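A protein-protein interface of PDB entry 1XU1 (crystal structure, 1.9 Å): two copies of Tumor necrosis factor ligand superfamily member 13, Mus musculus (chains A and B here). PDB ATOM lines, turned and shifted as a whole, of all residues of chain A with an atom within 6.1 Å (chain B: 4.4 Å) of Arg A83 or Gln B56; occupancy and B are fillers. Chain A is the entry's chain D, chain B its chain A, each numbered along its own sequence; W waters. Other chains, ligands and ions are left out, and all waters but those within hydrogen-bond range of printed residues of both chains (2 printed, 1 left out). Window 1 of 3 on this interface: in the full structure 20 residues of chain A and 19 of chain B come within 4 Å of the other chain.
The guanidinium group (NE) of Arg A83 sits at hydrogen-bond distance from a ring nitrogen (ND1) of His B129. N of Ser B98 is in hydrogen-bond range of O of Ile A85, 2.9 Å away. OG of Ser B98 sits close to SG of Cys A84, at 3.7 Å. OG of Ser B127 is in hydrogen-bond range of NH2 of Arg A83 (3.3 Å). The backbone carbonyl oxygen of Ser B98 is in hydrogen-bond range of the guanidinium group of Arg A86 (2.9 Å). OG of Ser A101 lies within hydrogen-bond range of OE1 of Gln B56 (2.6 Å). NE2 of Gln B56 is in hydrogen-bond range of O of Arg A83 (2.8 Å).
The side-chain sulfur (SG) of Cys A84 sits at hydrogen-bond distance from the guanidinium group (NH2) of Arg A86 (3.8 Å). The backbone NH (N) of Leu B58 is in hydrogen-bond range of the backbone carbonyl oxygen (O) of Gly B130 (3.4 Å). The backbone carbonyl oxygen (O) of Val A70 lies within hydrogen-bond range of the backbone NH (N) of Leu A81 (2.8 Å). A ring nitrogen (ND1) of His B129 lies close to the side-chain hydroxyl of Ser B127 (3.1 Å). N of Val A70 lies within hydrogen-bond range of O of Phe A82 (2.9 Å). The backbone NH (N) of Tyr A100 sits at hydrogen-bond distance from the side-chain sulfur (SG) of Cys A84 (3.4 Å).
Among the printed residues, pairs that only touch across the chains: Ala A102 with Phe B132 (3.2 Å), Ala A102 with Tyr B100 (3.4 Å), Phe A82 with His B129 (3.5 Å), Leu A81 with His B129 (3.5 Å), Thr A80 with His B129 (3.6 Å), Tyr A100 with Tyr B100 (3.6 Å), Arg A83 with Leu B58 (3.7 Å), Ser A101 with Phe B132 (3.7 Å), Phe A82 with Phe B132 (3.7 Å) and Ile A85 with Leu B58 (3.8 Å).
Arg A83 touches just these residues of chain B: Gln B56, Leu B58, Ser B127 and His B129. Of the printed residues of chain B, Tyr A100 touches Tyr B100 (3.6 Å). Gln B56 touches two residues of chain A. Of the printed residues of chain A, His B129 touches Thr A80 (3.6 Å), Leu A81 (3.5 Å), Phe A82 (3.5 Å) and Arg A83 (2.9 Å). The nearest residue of chain A that does not touch Gln B56 is Tyr A100 (4.4 Å).
Of the 14 printed residues of chain B, 7 touch a printed residue of chain A. Printed residues of chain B that touch a printed residue of chain A: Gln B56, Leu B58, Ser B98, Tyr B100, Ser B127, His B129 and Phe B132. Hydrophobic or aromatic side chains of chain B within 4 Å of the printed part of chain A: Leu B58, Tyr B100, His B129 and Phe B132. Of the 13 printed residues of chain A, 10 touch a printed residue of chain B. Among the printed residues, 17 pairs touch across the chains.
Tyr B100 touches its own counterpart, Tyr A100. 2 positions are printed for both chains. Of the 17 pairs that touch across the chains among the printed residues, 1 has its exchanged pair printed and touching as well.
Water W2 bridges OG of Ser B125 (2.8 Å) and NH2 of Arg A83 (3.0 Å). Water W1 bridges the side-chain hydroxyl (OH) of Tyr A100 (2.9 Å) and the side-chain hydroxyl (OH) of Tyr B100 (3.0 Å).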
ATOM      1  N   GLN A  68     -15.803  15.994 -16.576  1.00  0.00           N
ATOM      2  CA  GLN A  68     -16.919  15.989 -17.494  1.00  0.00           C
ATOM      3  C   GLN A  68     -18.132  15.276 -16.899  1.00  0.00           C
ATOM      4  O   GLN A  68     -18.017  14.475 -15.959  1.00  0.00           O
ATOM      5  CB  GLN A  68     -16.491  15.421 -18.852  1.00  0.00           C
ATOM      6  CG  GLN A  68     -16.274  13.910 -18.898  1.00  0.00           C
ATOM      7  CD  GLN A  68     -14.831  13.498 -18.699  1.00  0.00           C
ATOM      8  OE1 GLN A  68     -14.011  14.289 -18.207  1.00  0.00           O
ATOM      9  NE2 GLN A  68     -14.505  12.263 -19.099  1.00  0.00           N
ATOM     10  N   VAL A  69     -19.299  15.621 -17.426  1.00  0.00           N
ATOM     11  CA  VAL A  69     -20.578  15.093 -16.984  1.00  0.00           C
ATOM     12  C   VAL A  69     -21.240  14.520 -18.235  1.00  0.00           C
ATOM     13  O   VAL A  69     -21.481  15.240 -19.212  1.00  0.00           O
ATOM     14  CB  VAL A  69     -21.475  16.213 -16.387  1.00  0.00           C
ATOM     15  CG1 VAL A  69     -22.843  15.678 -15.940  1.00  0.00           C
ATOM     16  CG2 VAL A  69     -20.762  16.953 -15.224  1.00  0.00           C
ATOM     17  N   VAL A  70     -21.533  13.232 -18.212  1.00  0.00           N
ATOM     18  CA  VAL A  70     -22.179  12.580 -19.349  1.00  0.00           C
ATOM     19  C   VAL A  70     -23.616  12.286 -18.957  1.00  0.00           C
ATOM     20  O   VAL A  70     -23.867  11.673 -17.920  1.00  0.00           O
ATOM     21  CB  VAL A  70     -21.440  11.304 -19.741  1.00  0.00           C
ATOM     22  CG1 VAL A  70     -22.132  10.617 -20.921  1.00  0.00           C
ATOM     23  CG2 VAL A  70     -19.982  11.622 -20.061  1.00  0.00           C
ATOM     24  N   THR A  80     -28.086  12.152 -15.263  1.00  0.00           N
ATOM     25  CA  THR A  80     -26.630  12.033 -15.345  1.00  0.00           C
ATOM     26  C   THR A  80     -26.248  10.557 -15.277  1.00  0.00           C
ATOM     27  O   THR A  80     -26.635   9.862 -14.335  1.00  0.00           O
ATOM     28  CB  THR A  80     -25.959  12.770 -14.170  1.00  0.00           C
ATOM     29  OG1 THR A  80     -26.354  14.150 -14.158  1.00  0.00           O
ATOM     30  CG2 THR A  80     -24.454  12.803 -14.339  1.00  0.00           C
ATOM     31  N   LEU A  81     -25.473  10.090 -16.252  1.00  0.00           N
ATOM     32  CA  LEU A  81     -25.007   8.712 -16.267  1.00  0.00           C
ATOM     33  C   LEU A  81     -23.736   8.548 -15.444  1.00  0.00           C
ATOM     34  O   LEU A  81     -23.682   7.687 -14.562  1.00  0.00           O
ATOM     35  CB  LEU A  81     -24.803   8.226 -17.694  1.00  0.00           C
ATOM     36  CG  LEU A  81     -26.036   8.392 -18.583  1.00  0.00           C
ATOM     37  CD1 LEU A  81     -25.711   7.922 -19.982  1.00  0.00           C
ATOM     38  CD2 LEU A  81     -27.236   7.650 -18.003  1.00  0.00           C
ATOM     39  N   PHE A  82     -22.723   9.361 -15.741  1.00  0.00           N
ATOM     40  CA  PHE A  82     -21.486   9.368 -14.969  1.00  0.00           C
ATOM     41  C   PHE A  82     -20.741  10.705 -15.042  1.00  0.00           C
ATOM     42  O   PHE A  82     -20.945  11.507 -15.952  1.00  0.00           O
ATOM     43  CB  PHE A  82     -20.573   8.189 -15.349  1.00  0.00           C
ATOM     44  CG  PHE A  82     -20.142   8.157 -16.787  1.00  0.00           C
ATOM     45  CD1 PHE A  82     -18.996   8.820 -17.203  1.00  0.00           C
ATOM     46  CD2 PHE A  82     -20.846   7.414 -17.718  1.00  0.00           C
ATOM     47  CE1 PHE A  82     -18.577   8.759 -18.517  1.00  0.00           C
ATOM     48  CE2 PHE A  82     -20.435   7.360 -19.049  1.00  0.00           C
ATOM     49  CZ  PHE A  82     -19.303   8.038 -19.450  1.00  0.00           C
ATOM     50  N   ARG A  83     -19.919  10.945 -14.026  1.00  0.00           N
ATOM     51  CA  ARG A  83     -19.043  12.108 -13.940  1.00  0.00           C
ATOM     52  C   ARG A  83     -17.613  11.627 -13.712  1.00  0.00           C
ATOM     53  O   ARG A  83     -17.394  10.589 -13.093  1.00  0.00           O
ATOM     54  CB  ARG A  83     -19.417  12.974 -12.746  1.00  0.00           C
ATOM     55  CG  ARG A  83     -20.754  13.641 -12.815  1.00  0.00           C
ATOM     56  CD  ARG A  83     -21.040  14.525 -11.612  1.00  0.00           C
ATOM     57  NE  ARG A  83     -21.420  13.732 -10.445  1.00  0.00           N
ATOM     58  CZ  ARG A  83     -21.051  13.963  -9.188  1.00  0.00           C
ATOM     59  NH1 ARG A  83     -20.272  14.986  -8.848  1.00  0.00           N
ATOM     60  NH2 ARG A  83     -21.479  13.144  -8.236  1.00  0.00           N
ATOM     61  N   CYS A  84     -16.648  12.391 -14.198  1.00  0.00           N
ATOM     62  CA  CYS A  84     -15.232  12.155 -13.922  1.00  0.00           C
ATOM     63  C   CYS A  84     -14.692  13.473 -13.367  1.00  0.00           C
ATOM     64  O   CYS A  84     -15.043  14.534 -13.880  1.00  0.00           O
ATOM     65  CB  CYS A  84     -14.529  11.749 -15.229  1.00  0.00           C
ATOM     66  SG  CYS A  84     -12.805  11.286 -15.049  1.00  0.00           S
ATOM     67  N   ILE A  85     -13.906  13.421 -12.294  1.00  0.00           N
ATOM     68  CA  ILE A  85     -13.392  14.626 -11.635  1.00  0.00           C
ATOM     69  C   ILE A  85     -11.902  14.460 -11.321  1.00  0.00           C
ATOM     70  O   ILE A  85     -11.490  13.432 -10.798  1.00  0.00           O
ATOM     71  CB  ILE A  85     -14.172  14.912 -10.341  1.00  0.00           C
ATOM     72  CG1 ILE A  85     -15.654  15.205 -10.655  1.00  0.00           C
ATOM     73  CG2 ILE A  85     -13.556  16.081  -9.586  1.00  0.00           C
ATOM     74  CD1 ILE A  85     -16.537  15.133  -9.463  1.00  0.00           C
ATOM     75  N   ARG A  86     -11.111  15.484 -11.639  1.00  0.00           N
ATOM     76  CA  ARG A  86      -9.679  15.519 -11.329  1.00  0.00           C
ATOM     77  C   ARG A  86      -9.311  16.863 -10.704  1.00  0.00           C
ATOM     78  O   ARG A  86      -9.651  17.923 -11.249  1.00  0.00           O
ATOM     79  CB  ARG A  86      -8.836  15.357 -12.603  1.00  0.00           C
ATOM     80  CG  ARG A  86      -8.828  13.972 -13.240  1.00  0.00           C
ATOM     81  CD  ARG A  86      -8.209  12.853 -12.375  1.00  0.00           C
ATOM     82  NE  ARG A  86      -9.179  11.763 -12.186  1.00  0.00           N
ATOM     83  CZ  ARG A  86      -9.301  10.705 -12.983  1.00  0.00           C
ATOM     84  NH1 ARG A  86      -8.494  10.532 -14.019  1.00  0.00           N
ATOM     85  NH2 ARG A  86     -10.229   9.791 -12.734  1.00  0.00           N
ATOM     86  N   TYR A 100     -10.911   9.764 -17.378  1.00  0.00           N
ATOM     87  CA  TYR A 100     -11.623   8.680 -18.058  1.00  0.00           C
ATOM     88  C   TYR A 100     -12.719   8.120 -17.148  1.00  0.00           C
ATOM     89  O   TYR A 100     -12.507   7.897 -15.947  1.00  0.00           O
ATOM     90  CB  TYR A 100     -10.650   7.557 -18.473  1.00  0.00           C
ATOM     91  CG  TYR A 100     -11.300   6.380 -19.205  1.00  0.00           C
ATOM     92  CD1 TYR A 100     -11.975   5.390 -18.503  1.00  0.00           C
ATOM     93  CD2 TYR A 100     -11.229   6.246 -20.598  1.00  0.00           C
ATOM     94  CE1 TYR A 100     -12.585   4.339 -19.151  1.00  0.00           C
ATOM     95  CE2 TYR A 100     -11.845   5.164 -21.252  1.00  0.00           C
ATOM     96  CZ  TYR A 100     -12.523   4.225 -20.514  1.00  0.00           C
ATOM     97  OH  TYR A 100     -13.128   3.132 -21.121  1.00  0.00           O
ATOM     98  N   SER A 101     -13.892   7.887 -17.726  1.00  0.00           N
ATOM     99  CA  SER A 101     -14.927   7.114 -17.058  1.00  0.00           C
ATOM    100  C   SER A 101     -15.777   6.367 -18.095  1.00  0.00           C
ATOM    101  O   SER A 101     -15.732   6.656 -19.282  1.00  0.00           O
ATOM    102  CB  SER A 101     -15.788   8.046 -16.208  1.00  0.00           C
ATOM    103  OG  SER A 101     -16.619   7.323 -15.329  1.00  0.00           O
ATOM    104  N   ALA A 102     -16.529   5.383 -17.632  1.00  0.00           N
ATOM    105  CA  ALA A 102     -17.327   4.548 -18.512  1.00  0.00           C
ATOM    106  C   ALA A 102     -18.340   3.772 -17.696  1.00  0.00           C
ATOM    107  O   ALA A 102     -18.182   3.611 -16.501  1.00  0.00           O
ATOM    108  CB  ALA A 102     -16.434   3.583 -19.284  1.00  0.00           C
ATOM    109  N   SER B  55     -15.166  -0.354 -11.993  1.00  0.00           N
ATOM    110  CA  SER B  55     -15.432   0.228 -10.688  1.00  0.00           C
ATOM    111  C   SER B  55     -14.951   1.675 -10.657  1.00  0.00           C
ATOM    112  O   SER B  55     -13.827   1.949 -11.056  1.00  0.00           O
ATOM    113  CB  SER B  55     -14.711  -0.587  -9.611  1.00  0.00           C
ATOM    114  OG  SER B  55     -14.752   0.065  -8.350  1.00  0.00           O
ATOM    115  N   GLN B  56     -15.823   2.587 -10.226  1.00  0.00           N
ATOM    116  CA  GLN B  56     -15.458   3.983  -9.986  1.00  0.00           C
ATOM    117  C   GLN B  56     -15.850   4.363  -8.572  1.00  0.00           C
ATOM    118  O   GLN B  56     -16.918   3.994  -8.101  1.00  0.00           O
ATOM    119  CB  GLN B  56     -16.153   4.947 -10.941  1.00  0.00           C
ATOM    120  CG  GLN B  56     -15.726   6.411 -10.693  1.00  0.00           C
ATOM    121  CD  GLN B  56     -16.093   7.331 -11.812  1.00  0.00           C
ATOM    122  OE1 GLN B  56     -15.569   7.196 -12.911  1.00  0.00           O
ATOM    123  NE2 GLN B  56     -16.988   8.291 -11.540  1.00  0.00           N
ATOM    124  N   VAL B  57     -14.974   5.097  -7.895  1.00  0.00           N
ATOM    125  CA  VAL B  57     -15.320   5.694  -6.613  1.00  0.00           C
ATOM    126  C   VAL B  57     -14.942   7.161  -6.701  1.00  0.00           C
ATOM    127  O   VAL B  57     -13.860   7.500  -7.200  1.00  0.00           O
ATOM    128  CB  VAL B  57     -14.557   5.017  -5.420  1.00  0.00           C
ATOM    129  CG1 VAL B  57     -14.924   5.692  -4.106  1.00  0.00           C
ATOM    130  CG2 VAL B  57     -14.858   3.512  -5.333  1.00  0.00           C
ATOM    131  N   LEU B  58     -15.841   8.029  -6.242  1.00  0.00           N
ATOM    132  CA  LEU B  58     -15.582   9.465  -6.173  1.00  0.00           C
ATOM    133  C   LEU B  58     -15.286   9.844  -4.721  1.00  0.00           C
ATOM    134  O   LEU B  58     -16.121   9.646  -3.828  1.00  0.00           O
ATOM    135  CB  LEU B  58     -16.775  10.249  -6.714  1.00  0.00           C
ATOM    136  CG  LEU B  58     -16.809  11.762  -6.478  1.00  0.00           C
ATOM    137  CD1 LEU B  58     -15.545  12.454  -7.020  1.00  0.00           C
ATOM    138  CD2 LEU B  58     -18.057  12.350  -7.119  1.00  0.00           C
ATOM    139  N   GLN B  68      -9.393   2.232  -4.296  1.00  0.00           N
ATOM    140  CA  GLN B  68     -10.148   1.019  -4.029  1.00  0.00           C
ATOM    141  C   GLN B  68      -9.404  -0.221  -4.516  1.00  0.00           C
ATOM    142  O   GLN B  68      -8.554  -0.155  -5.405  1.00  0.00           O
ATOM    143  CB  GLN B  68     -11.568   1.112  -4.632  1.00  0.00           C
ATOM    144  CG  GLN B  68     -11.662   0.990  -6.133  1.00  0.00           C
ATOM    145  CD  GLN B  68     -11.789   2.326  -6.843  1.00  0.00           C
ATOM    146  OE1 GLN B  68     -11.370   3.360  -6.306  1.00  0.00           O
ATOM    147  NE2 GLN B  68     -12.363   2.309  -8.062  1.00  0.00           N
ATOM    148  N   SER B  98     -12.181  11.368  -8.813  1.00  0.00           N
ATOM    149  CA  SER B  98     -12.721  10.044  -9.134  1.00  0.00           C
ATOM    150  C   SER B  98     -11.583   9.079  -9.435  1.00  0.00           C
ATOM    151  O   SER B  98     -10.512   9.483  -9.877  1.00  0.00           O
ATOM    152  CB  SER B  98     -13.744  10.089 -10.281  1.00  0.00           C
ATOM    153  OG  SER B  98     -13.226  10.669 -11.462  1.00  0.00           O
ATOM    154  N   CYS B  99     -11.834   7.799  -9.194  1.00  0.00           N
ATOM    155  CA  CYS B  99     -10.846   6.748  -9.366  1.00  0.00           C
ATOM    156  C   CYS B  99     -11.546   5.638 -10.114  1.00  0.00           C
ATOM    157  O   CYS B  99     -12.449   5.015  -9.576  1.00  0.00           O
ATOM    158  CB  CYS B  99     -10.350   6.241  -8.009  1.00  0.00           C
ATOM    159  SG  CYS B  99      -8.633   5.688  -8.068  1.00  0.00           S
ATOM    160  N   TYR B 100     -11.170   5.445 -11.376  1.00  0.00           N
ATOM    161  CA  TYR B 100     -11.767   4.423 -12.225  1.00  0.00           C
ATOM    162  C   TYR B 100     -10.733   3.345 -12.602  1.00  0.00           C
ATOM    163  O   TYR B 100      -9.573   3.645 -12.907  1.00  0.00           O
ATOM    164  CB  TYR B 100     -12.331   5.080 -13.489  1.00  0.00           C
ATOM    165  CG  TYR B 100     -13.036   4.127 -14.402  1.00  0.00           C
ATOM    166  CD1 TYR B 100     -12.322   3.319 -15.271  1.00  0.00           C
ATOM    167  CD2 TYR B 100     -14.422   4.024 -14.408  1.00  0.00           C
ATOM    168  CE1 TYR B 100     -12.962   2.417 -16.080  1.00  0.00           C
ATOM    169  CE2 TYR B 100     -15.059   3.126 -15.220  1.00  0.00           C
ATOM    170  CZ  TYR B 100     -14.325   2.329 -16.059  1.00  0.00           C
ATOM    171  OH  TYR B 100     -14.921   1.426 -16.914  1.00  0.00           O
ATOM    172  N   SER B 125     -18.454   9.673  -2.182  1.00  0.00           N
ATOM    173  CA  SER B 125     -19.772  10.050  -2.644  1.00  0.00           C
ATOM    174  C   SER B 125     -20.643   8.817  -2.845  1.00  0.00           C
ATOM    175  O   SER B 125     -20.200   7.818  -3.414  1.00  0.00           O
ATOM    176  CB  SER B 125     -19.655  10.799  -3.966  1.00  0.00           C
ATOM    177  OG  SER B 125     -20.938  11.123  -4.455  1.00  0.00           O
ATOM    178  N   SER B 127     -23.375   9.255  -4.561  1.00  0.00           N
ATOM    179  CA  SER B 127     -24.027   9.587  -5.822  1.00  0.00           C
ATOM    180  C   SER B 127     -23.909   8.435  -6.805  1.00  0.00           C
ATOM    181  O   SER B 127     -22.811   7.902  -6.993  1.00  0.00           O
ATOM    182  CB  SER B 127     -23.349  10.810  -6.455  1.00  0.00           C
ATOM    183  OG  SER B 127     -23.967  11.110  -7.679  1.00  0.00           O
ATOM    184  N   HIS B 129     -23.879   8.552  -9.989  1.00  0.00           N
ATOM    185  CA  HIS B 129     -23.037   8.920 -11.136  1.00  0.00           C
ATOM    186  C   HIS B 129     -21.597   9.238 -10.718  1.00  0.00           C
ATOM    187  O   HIS B 129     -20.738   9.480 -11.565  1.00  0.00           O
ATOM    188  CB  HIS B 129     -23.652  10.045 -11.985  1.00  0.00           C
ATOM    189  CG  HIS B 129     -24.407  11.069 -11.199  1.00  0.00           C
ATOM    190  ND1 HIS B 129     -23.790  12.143 -10.600  1.00  0.00           N
ATOM    191  CD2 HIS B 129     -25.730  11.189 -10.921  1.00  0.00           C
ATOM    192  CE1 HIS B 129     -24.697  12.884  -9.984  1.00  0.00           C
ATOM    193  NE2 HIS B 129     -25.883  12.326 -10.160  1.00  0.00           N
ATOM    194  N   GLY B 130     -21.313   9.183  -9.420  1.00  0.00           N
ATOM    195  CA  GLY B 130     -19.952   9.346  -8.935  1.00  0.00           C
ATOM    196  C   GLY B 130     -19.278   8.028  -8.576  1.00  0.00           C
ATOM    197  O   GLY B 130     -18.092   7.830  -8.830  1.00  0.00           O
ATOM    198  N   THR B 131     -20.038   7.139  -7.944  1.00  0.00           N
ATOM    199  CA  THR B 131     -19.543   5.875  -7.429  1.00  0.00           C
ATOM    200  C   THR B 131     -20.444   4.757  -7.956  1.00  0.00           C
ATOM    201  O   THR B 131     -21.653   4.820  -7.808  1.00  0.00           O
ATOM    202  CB  THR B 131     -19.555   5.924  -5.889  1.00  0.00           C
ATOM    203  OG1 THR B 131     -18.583   6.879  -5.430  1.00  0.00           O
ATOM    204  CG2 THR B 131     -19.110   4.607  -5.279  1.00  0.00           C
ATOM    205  N   PHE B 132     -19.850   3.773  -8.616  1.00  0.00           N
ATOM    206  CA  PHE B 132     -20.603   2.692  -9.238  1.00  0.00           C
ATOM    207  C   PHE B 132     -19.739   1.479  -9.541  1.00  0.00           C
ATOM    208  O   PHE B 132     -18.513   1.548  -9.542  1.00  0.00           O
ATOM    209  CB  PHE B 132     -21.356   3.178 -10.484  1.00  0.00           C
ATOM    210  CG  PHE B 132     -20.495   3.865 -11.501  1.00  0.00           C
ATOM    211  CD1 PHE B 132     -19.743   3.130 -12.399  1.00  0.00           C
ATOM    212  CD2 PHE B 132     -20.460   5.260 -11.575  1.00  0.00           C
ATOM    213  CE1 PHE B 132     -18.960   3.768 -13.368  1.00  0.00           C
ATOM    214  CE2 PHE B 132     -19.657   5.908 -12.530  1.00  0.00           C
ATOM    215  CZ  PHE B 132     -18.922   5.159 -13.427  1.00  0.00           C
HETATM  216  O   HOH W   1     -13.373   0.787 -19.415  1.00  0.00           O
HETATM  217  O   HOH W   2     -21.241  13.795  -5.348  1.00  0.00           O
